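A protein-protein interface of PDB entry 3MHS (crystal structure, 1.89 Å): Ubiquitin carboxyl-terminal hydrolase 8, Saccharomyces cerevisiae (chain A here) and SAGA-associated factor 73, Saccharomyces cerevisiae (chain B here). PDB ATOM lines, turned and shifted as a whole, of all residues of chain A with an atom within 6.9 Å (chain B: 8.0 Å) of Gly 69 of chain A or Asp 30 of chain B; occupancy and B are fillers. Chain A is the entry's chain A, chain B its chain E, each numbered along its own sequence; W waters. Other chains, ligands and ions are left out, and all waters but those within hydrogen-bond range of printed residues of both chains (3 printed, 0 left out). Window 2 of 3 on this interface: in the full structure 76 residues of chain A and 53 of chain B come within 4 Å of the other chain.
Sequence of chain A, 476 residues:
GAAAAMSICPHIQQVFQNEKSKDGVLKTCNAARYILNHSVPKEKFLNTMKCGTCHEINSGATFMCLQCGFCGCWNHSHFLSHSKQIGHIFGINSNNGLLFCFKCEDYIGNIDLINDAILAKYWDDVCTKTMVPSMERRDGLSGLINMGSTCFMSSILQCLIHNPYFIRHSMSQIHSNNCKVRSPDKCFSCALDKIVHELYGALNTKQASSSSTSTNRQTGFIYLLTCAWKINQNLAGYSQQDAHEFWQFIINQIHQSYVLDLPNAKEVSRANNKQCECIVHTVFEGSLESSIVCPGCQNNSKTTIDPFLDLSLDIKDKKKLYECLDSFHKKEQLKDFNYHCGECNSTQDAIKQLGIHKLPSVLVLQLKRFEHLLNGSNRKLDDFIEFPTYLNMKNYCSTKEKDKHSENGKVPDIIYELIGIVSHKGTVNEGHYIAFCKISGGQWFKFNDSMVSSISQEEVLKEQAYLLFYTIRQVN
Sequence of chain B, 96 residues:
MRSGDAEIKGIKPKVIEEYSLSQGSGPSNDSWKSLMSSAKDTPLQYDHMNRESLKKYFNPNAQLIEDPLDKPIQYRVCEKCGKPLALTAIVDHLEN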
ATOM      1  N   LEU A  46     -26.305  28.326  34.313  1.00  0.00           N
ATOM      2  CA  LEU A  46     -26.952  28.161  33.033  1.00  0.00           C
ATOM      3  C   LEU A  46     -26.400  26.999  32.225  1.00  0.00           C
ATOM      4  O   LEU A  46     -27.111  26.424  31.382  1.00  0.00           O
ATOM      5  CB  LEU A  46     -26.876  29.454  32.231  1.00  0.00           C
ATOM      6  CG  LEU A  46     -27.772  30.596  32.719  1.00  0.00           C
ATOM      7  CD1 LEU A  46     -27.597  31.839  31.812  1.00  0.00           C
ATOM      8  CD2 LEU A  46     -29.242  30.146  32.736  1.00  0.00           C
ATOM      9  N   ASN A  47     -25.157  26.631  32.509  1.00  0.00           N
ATOM     10  CA  ASN A  47     -24.438  25.656  31.701  1.00  0.00           C
ATOM     11  C   ASN A  47     -24.023  24.376  32.405  1.00  0.00           C
ATOM     12  O   ASN A  47     -23.653  23.404  31.746  1.00  0.00           O
ATOM     13  CB  ASN A  47     -23.230  26.339  31.077  1.00  0.00           C
ATOM     14  CG  ASN A  47     -23.634  27.422  30.110  1.00  0.00           C
ATOM     15  OD1 ASN A  47     -24.217  27.145  29.059  1.00  0.00           O
ATOM     16  ND2 ASN A  47     -23.323  28.659  30.453  1.00  0.00           N
ATOM     17  N   LYS A  50     -28.398  23.399  34.577  1.00  0.00           N
ATOM     18  CA  LYS A  50     -29.596  23.423  33.764  1.00  0.00           C
ATOM     19  C   LYS A  50     -29.824  22.059  33.134  1.00  0.00           C
ATOM     20  O   LYS A  50     -28.992  21.597  32.358  1.00  0.00           O
ATOM     21  CB  LYS A  50     -29.456  24.453  32.650  1.00  0.00           C
ATOM     22  CG  LYS A  50     -30.726  24.653  31.873  1.00  0.00           C
ATOM     23  CD  LYS A  50     -30.469  25.402  30.596  1.00  0.00           C
ATOM     24  CE  LYS A  50     -30.399  26.871  30.808  1.00  0.00           C
ATOM     25  NZ  LYS A  50     -30.698  27.570  29.497  1.00  0.00           N
ATOM     26  N   PHE A  63     -26.275  16.703  36.877  1.00  0.00           N
ATOM     27  CA  PHE A  63     -25.087  15.910  36.578  1.00  0.00           C
ATOM     28  C   PHE A  63     -24.541  16.219  35.187  1.00  0.00           C
ATOM     29  O   PHE A  63     -25.290  16.283  34.215  1.00  0.00           O
ATOM     30  CB  PHE A  63     -25.392  14.410  36.723  1.00  0.00           C
ATOM     31  CG  PHE A  63     -25.773  14.013  38.121  1.00  0.00           C
ATOM     32  CD1 PHE A  63     -24.831  13.534  39.001  1.00  0.00           C
ATOM     33  CD2 PHE A  63     -27.073  14.174  38.565  1.00  0.00           C
ATOM     34  CE1 PHE A  63     -25.175  13.206  40.287  1.00  0.00           C
ATOM     35  CE2 PHE A  63     -27.418  13.869  39.856  1.00  0.00           C
ATOM     36  CZ  PHE A  63     -26.471  13.387  40.717  1.00  0.00           C
ATOM     37  N   MET A  64     -23.232  16.423  35.107  1.00  0.00           N
ATOM     38  CA  MET A  64     -22.533  16.631  33.840  1.00  0.00           C
ATOM     39  C   MET A  64     -22.044  15.265  33.316  1.00  0.00           C
ATOM     40  O   MET A  64     -21.268  14.609  33.991  1.00  0.00           O
ATOM     41  CB  MET A  64     -21.332  17.556  34.045  1.00  0.00           C
ATOM     42  CG  MET A  64     -21.670  18.886  34.764  1.00  0.00           C
ATOM     43  SD  MET A  64     -20.305  19.721  35.645  1.00  0.00           S
ATOM     44  CE  MET A  64     -19.321  20.401  34.318  1.00  0.00           C
ATOM     45  N   CYS A  65     -22.467  14.854  32.121  1.00  0.00           N
ATOM     46  CA  CYS A  65     -22.098  13.524  31.615  1.00  0.00           C
ATOM     47  C   CYS A  65     -20.599  13.335  31.395  1.00  0.00           C
ATOM     48  O   CYS A  65     -19.903  14.214  30.884  1.00  0.00           O
ATOM     49  CB  CYS A  65     -22.847  13.147  30.338  1.00  0.00           C
ATOM     50  SG  CYS A  65     -22.639  11.426  29.951  1.00  0.00           S
ATOM     51  N   LEU A  66     -20.108  12.170  31.809  1.00  0.00           N
ATOM     52  CA  LEU A  66     -18.699  11.811  31.646  1.00  0.00           C
ATOM     53  C   LEU A  66     -18.314  11.524  30.197  1.00  0.00           C
ATOM     54  O   LEU A  66     -17.155  11.683  29.818  1.00  0.00           O
ATOM     55  CB  LEU A  66     -18.386  10.576  32.491  1.00  0.00           C
ATOM     56  CG  LEU A  66     -17.006  10.586  33.142  1.00  0.00           C
ATOM     57  CD1 LEU A  66     -16.952  11.662  34.180  1.00  0.00           C
ATOM     58  CD2 LEU A  66     -16.712   9.216  33.737  1.00  0.00           C
ATOM     59  N   GLN A  67     -19.287  11.110  29.392  1.00  0.00           N
ATOM     60  CA  GLN A  67     -19.028  10.635  28.032  1.00  0.00           C
ATOM     61  C   GLN A  67     -19.511  11.591  26.948  1.00  0.00           C
ATOM     62  O   GLN A  67     -19.058  11.507  25.817  1.00  0.00           O
ATOM     63  CB  GLN A  67     -19.661   9.252  27.816  1.00  0.00           C
ATOM     64  CG  GLN A  67     -19.015   8.155  28.660  1.00  0.00           C
ATOM     65  CD  GLN A  67     -19.754   6.839  28.571  1.00  0.00           C
ATOM     66  OE1 GLN A  67     -20.386   6.405  29.535  1.00  0.00           O
ATOM     67  NE2 GLN A  67     -19.702   6.204  27.404  1.00  0.00           N
ATOM     68  N   CYS A  68     -20.424  12.489  27.299  1.00  0.00           N
ATOM     69  CA  CYS A  68     -20.901  13.507  26.360  1.00  0.00           C
ATOM     70  C   CYS A  68     -21.126  14.848  27.075  1.00  0.00           C
ATOM     71  O   CYS A  68     -20.680  15.022  28.213  1.00  0.00           O
ATOM     72  CB  CYS A  68     -22.148  13.007  25.619  1.00  0.00           C
ATOM     73  SG  CYS A  68     -23.714  12.950  26.515  1.00  0.00           S
ATOM     74  N   GLY A  69     -21.793  15.792  26.410  1.00  0.00           N
ATOM     75  CA  GLY A  69     -21.957  17.139  26.944  1.00  0.00           C
ATOM     76  C   GLY A  69     -23.232  17.375  27.727  1.00  0.00           C
ATOM     77  O   GLY A  69     -23.451  18.462  28.243  1.00  0.00           O
ATOM     78  N   PHE A  70     -24.075  16.356  27.815  1.00  0.00           N
ATOM     79  CA  PHE A  70     -25.406  16.486  28.408  1.00  0.00           C
ATOM     80  C   PHE A  70     -25.336  16.737  29.931  1.00  0.00           C
ATOM     81  O   PHE A  70     -24.462  16.193  30.617  1.00  0.00           O
ATOM     82  CB  PHE A  70     -26.200  15.206  28.096  1.00  0.00           C
ATOM     83  CG  PHE A  70     -27.551  15.139  28.733  1.00  0.00           C
ATOM     84  CD1 PHE A  70     -28.635  15.777  28.156  1.00  0.00           C
ATOM     85  CD2 PHE A  70     -27.753  14.399  29.881  1.00  0.00           C
ATOM     86  CE1 PHE A  70     -29.878  15.713  28.740  1.00  0.00           C
ATOM     87  CE2 PHE A  70     -28.998  14.311  30.458  1.00  0.00           C
ATOM     88  CZ  PHE A  70     -30.063  14.980  29.889  1.00  0.00           C
ATOM     89  N   CYS A  71     -26.236  17.591  30.428  1.00  0.00           N
ATOM     90  CA  CYS A  71     -26.488  17.730  31.853  1.00  0.00           C
ATOM     91  C   CYS A  71     -27.901  17.262  32.174  1.00  0.00           C
ATOM     92  O   CYS A  71     -28.842  17.579  31.458  1.00  0.00           O
ATOM     93  CB  CYS A  71     -26.292  19.187  32.294  1.00  0.00           C
ATOM     94  SG  CYS A  71     -24.604  19.790  32.017  1.00  0.00           S
ATOM     95  N   HIS A  82     -30.991   9.328  30.625  1.00  0.00           N
ATOM     96  CA  HIS A  82     -29.850   9.478  29.694  1.00  0.00           C
ATOM     97  C   HIS A  82     -28.974   8.247  29.809  1.00  0.00           C
ATOM     98  O   HIS A  82     -28.466   7.750  28.806  1.00  0.00           O
ATOM     99  CB  HIS A  82     -29.032  10.747  30.048  1.00  0.00           C
ATOM    100  CG  HIS A  82     -27.798  10.980  29.209  1.00  0.00           C
ATOM    101  ND1 HIS A  82     -27.851  11.447  27.914  1.00  0.00           N
ATOM    102  CD2 HIS A  82     -26.480  10.924  29.526  1.00  0.00           C
ATOM    103  CE1 HIS A  82     -26.621  11.614  27.450  1.00  0.00           C
ATOM    104  NE2 HIS A  82     -25.766  11.336  28.421  1.00  0.00           N
ATOM    105  N   HIS A  88     -24.902   5.950  29.052  1.00  0.00           N
ATOM    106  CA  HIS A  88     -23.867   6.689  29.789  1.00  0.00           C
ATOM    107  C   HIS A  88     -24.207   6.641  31.272  1.00  0.00           C
ATOM    108  O   HIS A  88     -25.139   7.297  31.730  1.00  0.00           O
ATOM    109  CB  HIS A  88     -23.750   8.127  29.291  1.00  0.00           C
ATOM    110  CG  HIS A  88     -23.337   8.229  27.855  1.00  0.00           C
ATOM    111  ND1 HIS A  88     -23.372   9.414  27.153  1.00  0.00           N
ATOM    112  CD2 HIS A  88     -22.953   7.275  26.964  1.00  0.00           C
ATOM    113  CE1 HIS A  88     -22.973   9.200  25.911  1.00  0.00           C
ATOM    114  NE2 HIS A  88     -22.724   7.909  25.767  1.00  0.00           N
ATOM    115  N   PRO B  27     -35.113  18.146  23.857  1.00  0.00           N
ATOM    116  CA  PRO B  27     -33.753  17.909  24.354  1.00  0.00           C
ATOM    117  C   PRO B  27     -32.758  19.012  23.957  1.00  0.00           C
ATOM    118  O   PRO B  27     -32.741  19.456  22.809  1.00  0.00           O
ATOM    119  CB  PRO B  27     -33.381  16.567  23.709  1.00  0.00           C
ATOM    120  CG  PRO B  27     -34.694  15.845  23.590  1.00  0.00           C
ATOM    121  CD  PRO B  27     -35.708  16.925  23.271  1.00  0.00           C
ATOM    122  N   SER B  28     -31.953  19.462  24.917  1.00  0.00           N
ATOM    123  CA  SER B  28     -30.962  20.506  24.656  1.00  0.00           C
ATOM    124  C   SER B  28     -29.806  19.950  23.826  1.00  0.00           C
ATOM    125  O   SER B  28     -29.490  18.758  23.899  1.00  0.00           O
ATOM    126  CB  SER B  28     -30.423  21.085  25.968  1.00  0.00           C
ATOM    127  OG  SER B  28     -29.333  21.966  25.735  1.00  0.00           O
ATOM    128  N   ASN B  29     -29.187  20.824  23.039  1.00  0.00           N
ATOM    129  CA  ASN B  29     -28.029  20.460  22.228  1.00  0.00           C
ATOM    130  C   ASN B  29     -26.706  20.976  22.831  1.00  0.00           C
ATOM    131  O   ASN B  29     -25.612  20.619  22.368  1.00  0.00           O
ATOM    132  CB  ASN B  29     -28.199  21.028  20.818  1.00  0.00           C
ATOM    133  CG  ASN B  29     -27.495  20.201  19.767  1.00  0.00           C
ATOM    134  OD1 ASN B  29     -28.045  19.947  18.691  1.00  0.00           O
ATOM    135  ND2 ASN B  29     -26.278  19.761  20.072  1.00  0.00           N
ATOM    136  N   ASP B  30     -26.801  21.819  23.855  1.00  0.00           N
ATOM    137  CA  ASP B  30     -25.603  22.390  24.444  1.00  0.00           C
ATOM    138  C   ASP B  30     -24.771  21.312  25.130  1.00  0.00           C
ATOM    139  O   ASP B  30     -25.201  20.160  25.271  1.00  0.00           O
ATOM    140  CB  ASP B  30     -25.939  23.558  25.373  1.00  0.00           C
ATOM    141  CG  ASP B  30     -25.893  24.909  24.653  1.00  0.00           C
ATOM    142  OD1 ASP B  30     -24.863  25.226  24.006  1.00  0.00           O
ATOM    143  OD2 ASP B  30     -26.884  25.667  24.739  1.00  0.00           O
ATOM    144  N   SER B  31     -23.551  21.687  25.487  1.00  0.00           N
ATOM    145  CA  SER B  31     -22.563  20.772  26.031  1.00  0.00           C
ATOM    146  C   SER B  31     -21.894  21.455  27.206  1.00  0.00           C
ATOM    147  O   SER B  31     -21.517  22.616  27.085  1.00  0.00           O
ATOM    148  CB  SER B  31     -21.519  20.484  24.957  1.00  0.00           C
ATOM    149  OG  SER B  31     -20.379  19.865  25.503  1.00  0.00           O
ATOM    150  N   TRP B  32     -21.751  20.765  28.341  1.00  0.00           N
ATOM    151  CA  TRP B  32     -21.073  21.383  29.478  1.00  0.00           C
ATOM    152  C   TRP B  32     -19.638  21.755  29.145  1.00  0.00           C
ATOM    153  O   TRP B  32     -19.077  22.644  29.783  1.00  0.00           O
ATOM    154  CB  TRP B  32     -21.137  20.531  30.766  1.00  0.00           C
ATOM    155  CG  TRP B  32     -20.471  19.160  30.726  1.00  0.00           C
ATOM    156  CD1 TRP B  32     -21.087  17.934  30.531  1.00  0.00           C
ATOM    157  CD2 TRP B  32     -19.088  18.880  30.943  1.00  0.00           C
ATOM    158  NE1 TRP B  32     -20.153  16.920  30.602  1.00  0.00           N
ATOM    159  CE2 TRP B  32     -18.925  17.473  30.872  1.00  0.00           C
ATOM    160  CE3 TRP B  32     -17.965  19.677  31.208  1.00  0.00           C
ATOM    161  CZ2 TRP B  32     -17.681  16.863  31.019  1.00  0.00           C
ATOM    162  CZ3 TRP B  32     -16.720  19.058  31.376  1.00  0.00           C
ATOM    163  CH2 TRP B  32     -16.595  17.669  31.281  1.00  0.00           C
ATOM    164  N   LYS B  33     -19.045  21.053  28.186  1.00  0.00           N
ATOM    165  CA  LYS B  33     -17.663  21.289  27.780  1.00  0.00           C
ATOM    166  C   LYS B  33     -17.482  22.573  26.989  1.00  0.00           C
ATOM    167  O   LYS B  33     -16.350  22.951  26.696  1.00  0.00           O
ATOM    168  CB  LYS B  33     -17.143  20.145  26.925  1.00  0.00           C
ATOM    169  CG  LYS B  33     -16.882  18.860  27.689  1.00  0.00           C
ATOM    170  CD  LYS B  33     -16.510  17.717  26.755  1.00  0.00           C
ATOM    171  CE  LYS B  33     -16.444  16.392  27.530  1.00  0.00           C
ATOM    172  NZ  LYS B  33     -15.897  15.264  26.727  1.00  0.00           N
ATOM    173  N   SER B  34     -18.595  23.183  26.574  1.00  0.00           N
ATOM    174  CA  SER B  34     -18.565  24.510  25.962  1.00  0.00           C
ATOM    175  C   SER B  34     -17.958  25.542  26.932  1.00  0.00           C
ATOM    176  O   SER B  34     -17.489  26.580  26.505  1.00  0.00           O
ATOM    177  CB  SER B  34     -19.975  24.955  25.516  1.00  0.00           C
ATOM    178  OG  SER B  34     -20.812  25.295  26.627  1.00  0.00           O
HETATM  179  O   HOH W   1     -16.270  12.345  26.345  1.00  0.00           O
HETATM  180  O   HOH W   2     -22.022  28.058  26.593  1.00  0.00           O
HETATM  181  O   HOH W   3     -23.167  24.706  27.536  1.00  0.00           O
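The indole nitrogen (NE1) of Trp 32 of chain B lies within hydrogen-bond range of the backbone carbonyl oxygen (O) of Cys 65 of chain A. NE1 of Trp 32 of chain B is in hydrogen-bond range of O of Cys 68 of chain A (3.1 Å). N of Trp 32 of chain B is in hydrogen-bond range of O of Gly 69 of chain A (2.9 Å).
SG of Cys 71 of chain A sits at hydrogen-bond distance from O of Asn 47 of chain A. The side-chain sulfur (SG) of Cys 65 of chain A lies close to the backbone NH (N) of Gln 67 of chain A (3.4 Å). O of Phe 70 of chain A is in hydrogen-bond range of N of Cys 65 of chain A (2.8 Å). The side-chain sulfur (SG) of Cys 68 of chain A sits close to the backbone NH (N) of Phe 70 of chain A. The side-chain hydroxyl (OG) of Ser 28 of chain B is in hydrogen-bond range of the backbone NH (N) of Asp 30 of chain B, 3.2 Å away. The backbone NH (N) of Lys 33 of chain B lies close to the side-chain hydroxyl (OG) of Ser 31 of chain B (3.2 Å).
Among the printed residues, merely in contact across the chains: Asn 47 of chain A with Trp 32 of chain B (3.9 Å), Met 64 of chain A with Trp 32 of chain B (3.5 Å), Gly 69 of chain A with Asp 30 of chain B (3.8 Å), Gly 69 of chain A with Ser 31 of chain B (3.3 Å), Phe 70 of chain A with Trp 32 of chain B (3.8 Å) and Cys 71 of chain A with Trp 32 of chain B (3.8 Å).
Gly 69 of chain A touches just these residues of chain B: Asp 30 (3.8 Å), Ser 31 (3.3 Å) and Trp 32 (2.9 Å). Of chain A, only Gly 69 comes within 4 Å of Asp 30 of chain B. Cys 68 of chain A touches just one residue of chain B: Trp 32 (3.1 Å). Printed residues of chain A within 4 Å of Trp 32 of chain B: Asn 47 (3.9 Å), Met 64 (3.5 Å), Cys 65 (2.7 Å), Cys 68 (3.1 Å), Gly 69 (2.9 Å), Phe 70 (3.8 Å) and Cys 71 (3.8 Å). Of the printed residues of chain B, Phe 70 of chain A touches Trp 32 (3.8 Å). Of the printed residues of chain B, Met 64 of chain A touches Trp 32. Ser 34 of chain B touches none of the printed residues of chain A. Lys 33 of chain B touches none of the printed residues of chain A. The nearest residue of chain B that does not touch Gly 69 of chain A is Lys 33 of chain B (5.0 Å). The nearest residue of chain A that does not touch Asp 30 of chain B is Phe 70 of chain A (4.7 Å). The nearest printed residue of chain B that does not touch Cys 71 of chain A is Ser 31 of chain B (5.8 Å).
Along chain A the printed residues that touch a printed residue of chain B span positions 47 to 71. Printed residues of chain B that touch a printed residue of chain A: Asp 30, Ser 31 and Trp 32. Hydrophobic or aromatic side chains of chain B within 4 Å of the printed part of chain A: Trp 32. Among the printed residues, 9 pairs touch across the chains. Among the printed residues, no Asp or Glu carboxylate lies within 4 Å of a Lys or Arg side-chain nitrogen of the other chain.
Water W3 lies within hydrogen-bond range of OG of Ser 34 of chain B, O of Ser 31 of chain B and OD1 of Asn 47 of chain A. Water W1 lies within hydrogen-bond range of the backbone carbonyl oxygen of Gln 67 of chain A (3.0 Å) and the side-chain amino group of Lys 33 of chain B (3.0 Å). Water W2 bridges the side-chain hydroxyl (OG) of Ser 34 of chain B and the side-chain amide oxygen (OD1) of Asn 47 of chain A.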
